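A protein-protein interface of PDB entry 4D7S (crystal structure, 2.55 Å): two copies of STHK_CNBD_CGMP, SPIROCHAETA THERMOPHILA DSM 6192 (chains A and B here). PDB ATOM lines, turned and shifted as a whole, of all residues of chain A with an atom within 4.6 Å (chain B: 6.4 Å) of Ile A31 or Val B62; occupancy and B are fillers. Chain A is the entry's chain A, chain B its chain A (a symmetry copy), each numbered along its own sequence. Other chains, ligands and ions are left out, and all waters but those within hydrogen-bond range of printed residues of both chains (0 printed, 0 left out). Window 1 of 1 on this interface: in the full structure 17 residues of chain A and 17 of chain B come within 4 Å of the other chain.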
ATOM      1  N   VAL A  14     -32.434 -32.407 -20.488  1.00  0.00           N
ATOM      2  CA  VAL A  14     -32.227 -31.931 -19.125  1.00  0.00           C
ATOM      3  C   VAL A  14     -32.012 -30.421 -19.119  1.00  0.00           C
ATOM      4  O   VAL A  14     -32.539 -29.715 -18.256  1.00  0.00           O
ATOM      5  CB  VAL A  14     -31.031 -32.644 -18.456  1.00  0.00           C
ATOM      6  CG1 VAL A  14     -30.636 -31.947 -17.165  1.00  0.00           C
ATOM      7  CG2 VAL A  14     -31.373 -34.098 -18.182  1.00  0.00           C
ATOM      8  N   LEU A  18     -34.171 -27.418 -17.450  1.00  0.00           N
ATOM      9  CA  LEU A  18     -33.579 -26.406 -16.587  1.00  0.00           C
ATOM     10  C   LEU A  18     -33.988 -24.985 -16.949  1.00  0.00           C
ATOM     11  O   LEU A  18     -34.097 -24.126 -16.075  1.00  0.00           O
ATOM     12  CB  LEU A  18     -32.057 -26.505 -16.638  1.00  0.00           C
ATOM     13  CG  LEU A  18     -31.417 -27.706 -15.950  1.00  0.00           C
ATOM     14  CD1 LEU A  18     -29.900 -27.645 -16.110  1.00  0.00           C
ATOM     15  CD2 LEU A  18     -31.836 -27.797 -14.492  1.00  0.00           C
ATOM     16  N   ILE A  23     -33.902 -22.442 -13.755  1.00  0.00           N
ATOM     17  CA  ILE A  23     -32.961 -22.787 -12.703  1.00  0.00           C
ATOM     18  C   ILE A  23     -31.815 -21.775 -12.702  1.00  0.00           C
ATOM     19  O   ILE A  23     -31.359 -21.330 -13.759  1.00  0.00           O
ATOM     20  CB  ILE A  23     -32.421 -24.226 -12.876  1.00  0.00           C
ATOM     21  CG1 ILE A  23     -33.548 -25.250 -12.721  1.00  0.00           C
ATOM     22  CG2 ILE A  23     -31.362 -24.529 -11.848  1.00  0.00           C
ATOM     23  CD1 ILE A  23     -34.164 -25.280 -11.333  1.00  0.00           C
ATOM     24  N   LEU A  27     -26.613 -22.971 -10.510  1.00  0.00           N
ATOM     25  CA  LEU A  27     -26.990 -24.382 -10.490  1.00  0.00           C
ATOM     26  C   LEU A  27     -26.926 -24.996 -11.892  1.00  0.00           C
ATOM     27  O   LEU A  27     -26.496 -26.137 -12.051  1.00  0.00           O
ATOM     28  CB  LEU A  27     -28.384 -24.568  -9.881  1.00  0.00           C
ATOM     29  CG  LEU A  27     -28.834 -26.022  -9.697  1.00  0.00           C
ATOM     30  CD1 LEU A  27     -27.741 -26.845  -9.038  1.00  0.00           C
ATOM     31  CD2 LEU A  27     -30.112 -26.096  -8.876  1.00  0.00           C
ATOM     32  N   GLN A  28     -27.346 -24.239 -12.904  1.00  0.00           N
ATOM     33  CA  GLN A  28     -27.288 -24.722 -14.286  1.00  0.00           C
ATOM     34  C   GLN A  28     -25.856 -25.030 -14.700  1.00  0.00           C
ATOM     35  O   GLN A  28     -25.606 -26.017 -15.383  1.00  0.00           O
ATOM     36  CB  GLN A  28     -27.901 -23.713 -15.260  1.00  0.00           C
ATOM     37  CG  GLN A  28     -29.356 -23.387 -14.999  1.00  0.00           C
ATOM     38  CD  GLN A  28     -30.116 -23.047 -16.271  1.00  0.00           C
ATOM     39  OE1 GLN A  28     -29.716 -23.438 -17.368  1.00  0.00           O
ATOM     40  NE2 GLN A  28     -31.219 -22.320 -16.126  1.00  0.00           N
ATOM     41  N   ARG A  29     -24.916 -24.189 -14.279  1.00  0.00           N
ATOM     42  CA  ARG A  29     -23.520 -24.398 -14.632  1.00  0.00           C
ATOM     43  C   ARG A  29     -22.964 -25.626 -13.929  1.00  0.00           C
ATOM     44  O   ARG A  29     -22.225 -26.404 -14.525  1.00  0.00           O
ATOM     45  CB  ARG A  29     -22.677 -23.178 -14.259  1.00  0.00           C
ATOM     46  CG  ARG A  29     -21.250 -23.220 -14.796  1.00  0.00           C
ATOM     47  CD  ARG A  29     -20.348 -22.267 -14.027  1.00  0.00           C
ATOM     48  NE  ARG A  29     -20.344 -22.568 -12.596  1.00  0.00           N
ATOM     49  CZ  ARG A  29     -19.630 -23.537 -12.029  1.00  0.00           C
ATOM     50  NH1 ARG A  29     -18.849 -24.310 -12.772  1.00  0.00           N
ATOM     51  NH2 ARG A  29     -19.700 -23.734 -10.718  1.00  0.00           N
ATOM     52  N   ARG A  30     -23.333 -25.795 -12.665  1.00  0.00           N
ATOM     53  CA  ARG A  30     -22.969 -26.981 -11.895  1.00  0.00           C
ATOM     54  C   ARG A  30     -23.407 -28.268 -12.594  1.00  0.00           C
ATOM     55  O   ARG A  30     -22.649 -29.236 -12.674  1.00  0.00           O
ATOM     56  CB  ARG A  30     -23.578 -26.889 -10.497  1.00  0.00           C
ATOM     57  CG  ARG A  30     -22.943 -25.800  -9.646  1.00  0.00           C
ATOM     58  CD  ARG A  30     -23.664 -25.635  -8.329  1.00  0.00           C
ATOM     59  NE  ARG A  30     -23.798 -26.904  -7.628  1.00  0.00           N
ATOM     60  CZ  ARG A  30     -24.584 -27.093  -6.574  1.00  0.00           C
ATOM     61  NH1 ARG A  30     -25.316 -26.092  -6.100  1.00  0.00           N
ATOM     62  NH2 ARG A  30     -24.645 -28.287  -6.001  1.00  0.00           N
ATOM     63  N   ILE A  31     -24.634 -28.262 -13.103  1.00  0.00           N
ATOM     64  CA  ILE A  31     -25.203 -29.434 -13.754  1.00  0.00           C
ATOM     65  C   ILE A  31     -24.491 -29.729 -15.074  1.00  0.00           C
ATOM     66  O   ILE A  31     -24.138 -30.876 -15.354  1.00  0.00           O
ATOM     67  CB  ILE A  31     -26.713 -29.248 -13.996  1.00  0.00           C
ATOM     68  CG1 ILE A  31     -27.458 -29.228 -12.661  1.00  0.00           C
ATOM     69  CG2 ILE A  31     -27.259 -30.347 -14.888  1.00  0.00           C
ATOM     70  CD1 ILE A  31     -28.921 -28.912 -12.792  1.00  0.00           C
ATOM     71  N   LEU A  32     -24.269 -28.692 -15.879  1.00  0.00           N
ATOM     72  CA  LEU A  32     -23.538 -28.848 -17.134  1.00  0.00           C
ATOM     73  C   LEU A  32     -22.096 -29.271 -16.881  1.00  0.00           C
ATOM     74  O   LEU A  32     -21.536 -30.077 -17.624  1.00  0.00           O
ATOM     75  CB  LEU A  32     -23.557 -27.554 -17.949  1.00  0.00           C
ATOM     76  CG  LEU A  32     -24.918 -26.921 -18.239  1.00  0.00           C
ATOM     77  CD1 LEU A  32     -24.774 -25.740 -19.192  1.00  0.00           C
ATOM     78  CD2 LEU A  32     -25.887 -27.955 -18.778  1.00  0.00           C
ATOM     79  N   GLU A  33     -21.500 -28.711 -15.835  1.00  0.00           N
ATOM     80  CA  GLU A  33     -20.134 -29.047 -15.456  1.00  0.00           C
ATOM     81  C   GLU A  33     -20.041 -30.496 -14.987  1.00  0.00           C
ATOM     82  O   GLU A  33     -19.031 -31.167 -15.206  1.00  0.00           O
ATOM     83  CB  GLU A  33     -19.644 -28.100 -14.361  1.00  0.00           C
ATOM     84  CG  GLU A  33     -18.148 -28.077 -14.156  1.00  0.00           C
ATOM     85  CD  GLU A  33     -17.739 -27.104 -13.069  1.00  0.00           C
ATOM     86  OE1 GLU A  33     -18.293 -27.194 -11.952  1.00  0.00           O
ATOM     87  OE2 GLU A  33     -16.874 -26.242 -13.335  1.00  0.00           O
ATOM     88  N   TYR A  34     -21.106 -30.973 -14.350  1.00  0.00           N
ATOM     89  CA  TYR A  34     -21.169 -32.354 -13.889  1.00  0.00           C
ATOM     90  C   TYR A  34     -21.218 -33.316 -15.064  1.00  0.00           C
ATOM     91  O   TYR A  34     -20.521 -34.327 -15.081  1.00  0.00           O
ATOM     92  CB  TYR A  34     -22.387 -32.578 -12.991  1.00  0.00           C
ATOM     93  CG  TYR A  34     -22.686 -34.043 -12.753  1.00  0.00           C
ATOM     94  CD1 TYR A  34     -21.957 -34.777 -11.828  1.00  0.00           C
ATOM     95  CD2 TYR A  34     -23.688 -34.695 -13.465  1.00  0.00           C
ATOM     96  CE1 TYR A  34     -22.220 -36.115 -11.611  1.00  0.00           C
ATOM     97  CE2 TYR A  34     -23.955 -36.034 -13.256  1.00  0.00           C
ATOM     98  CZ  TYR A  34     -23.218 -36.738 -12.326  1.00  0.00           C
ATOM     99  OH  TYR A  34     -23.479 -38.070 -12.108  1.00  0.00           O
ATOM    100  N   PHE A  35     -22.061 -33.002 -16.036  1.00  0.00           N
ATOM    101  CA  PHE A  35     -22.246 -33.874 -17.184  1.00  0.00           C
ATOM    102  C   PHE A  35     -21.033 -33.875 -18.119  1.00  0.00           C
ATOM    103  O   PHE A  35     -20.769 -34.871 -18.795  1.00  0.00           O
ATOM    104  CB  PHE A  35     -23.509 -33.482 -17.939  1.00  0.00           C
ATOM    105  CG  PHE A  35     -24.777 -33.976 -17.300  1.00  0.00           C
ATOM    106  CD1 PHE A  35     -25.072 -35.331 -17.279  1.00  0.00           C
ATOM    107  CD2 PHE A  35     -25.683 -33.092 -16.740  1.00  0.00           C
ATOM    108  CE1 PHE A  35     -26.239 -35.793 -16.694  1.00  0.00           C
ATOM    109  CE2 PHE A  35     -26.850 -33.549 -16.156  1.00  0.00           C
ATOM    110  CZ  PHE A  35     -27.130 -34.899 -16.134  1.00  0.00           C
ATOM    111  N   LEU B  51     -34.893 -35.600 -13.016  1.00  0.00           N
ATOM    112  CA  LEU B  51     -34.112 -35.536 -11.788  1.00  0.00           C
ATOM    113  C   LEU B  51     -33.401 -36.862 -11.575  1.00  0.00           C
ATOM    114  O   LEU B  51     -32.359 -36.907 -10.926  1.00  0.00           O
ATOM    115  CB  LEU B  51     -34.961 -35.159 -10.569  1.00  0.00           C
ATOM    116  CG  LEU B  51     -35.136 -33.653 -10.310  1.00  0.00           C
ATOM    117  CD1 LEU B  51     -35.933 -32.921 -11.389  1.00  0.00           C
ATOM    118  CD2 LEU B  51     -35.698 -33.365  -8.910  1.00  0.00           C
ATOM    119  N   LEU B  54     -29.704 -36.912 -12.286  1.00  0.00           N
ATOM    120  CA  LEU B  54     -28.757 -36.181 -11.445  1.00  0.00           C
ATOM    121  C   LEU B  54     -28.338 -36.972 -10.199  1.00  0.00           C
ATOM    122  O   LEU B  54     -29.096 -37.812  -9.717  1.00  0.00           O
ATOM    123  CB  LEU B  54     -29.368 -34.844 -11.024  1.00  0.00           C
ATOM    124  CG  LEU B  54     -30.012 -33.987 -12.109  1.00  0.00           C
ATOM    125  CD1 LEU B  54     -30.915 -32.951 -11.465  1.00  0.00           C
ATOM    126  CD2 LEU B  54     -28.950 -33.320 -12.967  1.00  0.00           C
ATOM    127  N   PRO B  57     -26.765 -34.550  -4.642  1.00  0.00           N
ATOM    128  CA  PRO B  57     -26.612 -33.128  -4.330  1.00  0.00           C
ATOM    129  C   PRO B  57     -27.240 -32.216  -5.362  1.00  0.00           C
ATOM    130  O   PRO B  57     -27.704 -31.131  -5.018  1.00  0.00           O
ATOM    131  CB  PRO B  57     -25.091 -32.925  -4.311  1.00  0.00           C
ATOM    132  CG  PRO B  57     -24.493 -34.256  -4.230  1.00  0.00           C
ATOM    133  CD  PRO B  57     -25.447 -35.173  -4.882  1.00  0.00           C
ATOM    134  N   LEU B  58     -27.235 -32.640  -6.617  1.00  0.00           N
ATOM    135  CA  LEU B  58     -27.782 -31.808  -7.670  1.00  0.00           C
ATOM    136  C   LEU B  58     -29.296 -31.957  -7.730  1.00  0.00           C
ATOM    137  O   LEU B  58     -29.992 -31.015  -8.091  1.00  0.00           O
ATOM    138  CB  LEU B  58     -27.130 -32.136  -9.017  1.00  0.00           C
ATOM    139  CG  LEU B  58     -25.653 -31.721  -9.099  1.00  0.00           C
ATOM    140  CD1 LEU B  58     -25.030 -32.118 -10.428  1.00  0.00           C
ATOM    141  CD2 LEU B  58     -25.501 -30.221  -8.863  1.00  0.00           C
ATOM    142  N   ARG B  59     -29.813 -33.126  -7.354  1.00  0.00           N
ATOM    143  CA  ARG B  59     -31.262 -33.293  -7.289  1.00  0.00           C
ATOM    144  C   ARG B  59     -31.819 -32.527  -6.103  1.00  0.00           C
ATOM    145  O   ARG B  59     -32.887 -31.913  -6.189  1.00  0.00           O
ATOM    146  CB  ARG B  59     -31.668 -34.761  -7.152  1.00  0.00           C
ATOM    147  CG  ARG B  59     -31.152 -35.673  -8.221  1.00  0.00           C
ATOM    148  CD  ARG B  59     -31.607 -37.108  -7.988  1.00  0.00           C
ATOM    149  NE  ARG B  59     -31.682 -37.473  -6.579  1.00  0.00           N
ATOM    150  CZ  ARG B  59     -31.063 -38.528  -6.062  1.00  0.00           C
ATOM    151  NH1 ARG B  59     -30.312 -39.294  -6.839  1.00  0.00           N
ATOM    152  NH2 ARG B  59     -31.177 -38.804  -4.770  1.00  0.00           N
ATOM    153  N   LEU B  60     -31.087 -32.585  -4.994  1.00  0.00           N
ATOM    154  CA  LEU B  60     -31.407 -31.814  -3.804  1.00  0.00           C
ATOM    155  C   LEU B  60     -31.493 -30.324  -4.127  1.00  0.00           C
ATOM    156  O   LEU B  60     -32.439 -29.644  -3.728  1.00  0.00           O
ATOM    157  CB  LEU B  60     -30.358 -32.066  -2.724  1.00  0.00           C
ATOM    158  CG  LEU B  60     -30.779 -31.822  -1.279  1.00  0.00           C
ATOM    159  CD1 LEU B  60     -31.966 -32.701  -0.916  1.00  0.00           C
ATOM    160  CD2 LEU B  60     -29.616 -32.063  -0.327  1.00  0.00           C
ATOM    161  N   ALA B  61     -30.499 -29.829  -4.858  1.00  0.00           N
ATOM    162  CA  ALA B  61     -30.435 -28.422  -5.230  1.00  0.00           C
ATOM    163  C   ALA B  61     -31.583 -28.023  -6.154  1.00  0.00           C
ATOM    164  O   ALA B  61     -32.234 -27.000  -5.941  1.00  0.00           O
ATOM    165  CB  ALA B  61     -29.095 -28.114  -5.883  1.00  0.00           C
ATOM    166  N   VAL B  62     -31.825 -28.833  -7.180  1.00  0.00           N
ATOM    167  CA  VAL B  62     -32.897 -28.556  -8.128  1.00  0.00           C
ATOM    168  C   VAL B  62     -34.263 -28.594  -7.450  1.00  0.00           C
ATOM    169  O   VAL B  62     -35.087 -27.706  -7.660  1.00  0.00           O
ATOM    170  CB  VAL B  62     -32.880 -29.552  -9.309  1.00  0.00           C
ATOM    171  CG1 VAL B  62     -34.106 -29.361 -10.183  1.00  0.00           C
ATOM    172  CG2 VAL B  62     -31.606 -29.387 -10.131  1.00  0.00           C
ATOM    173  N   ALA B  63     -34.486 -29.610  -6.618  1.00  0.00           N
ATOM    174  CA  ALA B  63     -35.742 -29.753  -5.887  1.00  0.00           C
ATOM    175  C   ALA B  63     -36.017 -28.540  -5.004  1.00  0.00           C
ATOM    176  O   ALA B  63     -37.148 -28.067  -4.924  1.00  0.00           O
ATOM    177  CB  ALA B  63     -35.730 -31.026  -5.047  1.00  0.00           C
ATOM    178  N   MET B  64     -34.979 -28.029  -4.351  1.00  0.00           N
ATOM    179  CA  MET B  64     -35.138 -26.883  -3.463  1.00  0.00           C
ATOM    180  C   MET B  64     -35.361 -25.577  -4.229  1.00  0.00           C
ATOM    181  O   MET B  64     -35.818 -24.590  -3.655  1.00  0.00           O
ATOM    182  CB  MET B  64     -33.917 -26.747  -2.544  1.00  0.00           C
ATOM    183  CG  MET B  64     -33.810 -27.837  -1.487  1.00  0.00           C
ATOM    184  SD  MET B  64     -32.490 -27.561  -0.287  1.00  0.00           S
ATOM    185  CE  MET B  64     -32.944 -25.956   0.360  1.00  0.00           C
ATOM    186  N   GLU B  65     -35.047 -25.571  -5.523  1.00  0.00           N
ATOM    187  CA  GLU B  65     -35.303 -24.398  -6.354  1.00  0.00           C
ATOM    188  C   GLU B  65     -36.711 -24.421  -6.939  1.00  0.00           C
ATOM    189  O   GLU B  65     -37.449 -23.443  -6.821  1.00  0.00           O
ATOM    190  CB  GLU B  65     -34.267 -24.287  -7.479  1.00  0.00           C
ATOM    191  CG  GLU B  65     -32.925 -23.728  -7.024  1.00  0.00           C
ATOM    192  CD  GLU B  65     -32.206 -22.952  -8.114  1.00  0.00           C
ATOM    193  OE1 GLU B  65     -32.846 -22.611  -9.130  1.00  0.00           O
ATOM    194  OE2 GLU B  65     -31.000 -22.672  -7.950  1.00  0.00           O
ATOM    195  N   ILE B  66     -37.076 -25.534  -7.571  1.00  0.00           N
ATOM    196  CA  ILE B  66     -38.376 -25.653  -8.227  1.00  0.00           C
ATOM    197  C   ILE B  66     -39.528 -25.746  -7.224  1.00  0.00           C
ATOM    198  O   ILE B  66     -40.663 -25.393  -7.539  1.00  0.00           O
ATOM    199  CB  ILE B  66     -38.431 -26.875  -9.168  1.00  0.00           C
ATOM    200  CG1 ILE B  66     -38.136 -28.162  -8.397  1.00  0.00           C
ATOM    201  CG2 ILE B  66     -37.460 -26.700 -10.329  1.00  0.00           C
ATOM    202  CD1 ILE B  66     -37.877 -29.359  -9.284  1.00  0.00           C
ATOM    203  N   HIS B  67     -39.234 -26.221  -6.019  1.00  0.00           N
ATOM    204  CA  HIS B  67     -40.263 -26.406  -5.000  1.00  0.00           C
ATOM    205  C   HIS B  67     -40.038 -25.495  -3.797  1.00  0.00           C
ATOM    206  O   HIS B  67     -40.348 -25.858  -2.664  1.00  0.00           O
ATOM    207  CB  HIS B  67     -40.310 -27.868  -4.551  1.00  0.00           C
ATOM    208  CG  HIS B  67     -40.593 -28.834  -5.663  1.00  0.00           C
ATOM    209  ND1 HIS B  67     -41.681 -28.709  -6.494  1.00  0.00           N
ATOM    210  CD2 HIS B  67     -39.932 -29.945  -6.065  1.00  0.00           C
ATOM    211  CE1 HIS B  67     -41.679 -29.701  -7.372  1.00  0.00           C
ATOM    212  NE2 HIS B  67     -40.630 -30.463  -7.133  1.00  0.00           N
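Among the printed residues, pairs that only touch across the chains: Arg A30 with Leu B58 (3.6 Å), Ile A23 with Glu B65 (3.6 Å), Leu A27 with Ala B61 (3.6 Å), Leu A27 with Val B62 (3.6 Å), Leu A27 with Glu B65 (3.7 Å), Tyr A34 with Leu B58 (3.7 Å), Ile A23 with Ile B66 (3.7 Å), Ile A31 with Val B62 (3.8 Å), Phe A35 with Leu B54 (3.8 Å) and Ile A31 with Leu B54 (3.9 Å).
Hydrophobic or aromatic side chains of chain A that line the printed part of chain B: Ile A23, Leu A27, Ile A31, Tyr A34 and Phe A35. Of the 13 printed residues of chain B, 6 touch a printed residue of chain A. Hydrophobic or aromatic side chains of chain B that line the printed part of chain A: Leu B54, Leu B58, Ala B61, Val B62 and Ile B66. Among the printed residues, no Asp or Glu carboxylate lies within 4 Å of a Lys or Arg side-chain nitrogen of the other chain.
Printed residues of chain B within 4 Å of Ile A23: Glu B65 and Ile B66. Of chain B, only Leu B54 and Val B62 come within 4 Å of Ile A31. Of the printed residues of chain B, Phe A35 touches Leu B54. Printed residues of chain A within 4 Å of Leu B54: Ile A31 and Phe A35. Pro B57 touches none of the printed residues of chain A. Of the printed residues of chain A, Leu B58 touches Arg A30 and Tyr A34. Printed residues of chain A within 4 Å of Val B62: Leu A27 and Ile A31. The nearest residue of chain A that does not touch Val B62 is Ile A23 (4.2 Å).
O of Leu A18 sits at hydrogen-bond distance from N of Ile A23, 2.9 Å away. O of Ile A23 lies within hydrogen-bond range of NE2 of Gln A28. The guanidinium group (NH1) of Arg B59 sits close to the backbone carbonyl oxygen (O) of Leu B54, 3.5 Å away.
No position is printed for both chains. Of the 10 pairs that touch across the chains among the printed residues, none has its exchanged pair printed and touching as well.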
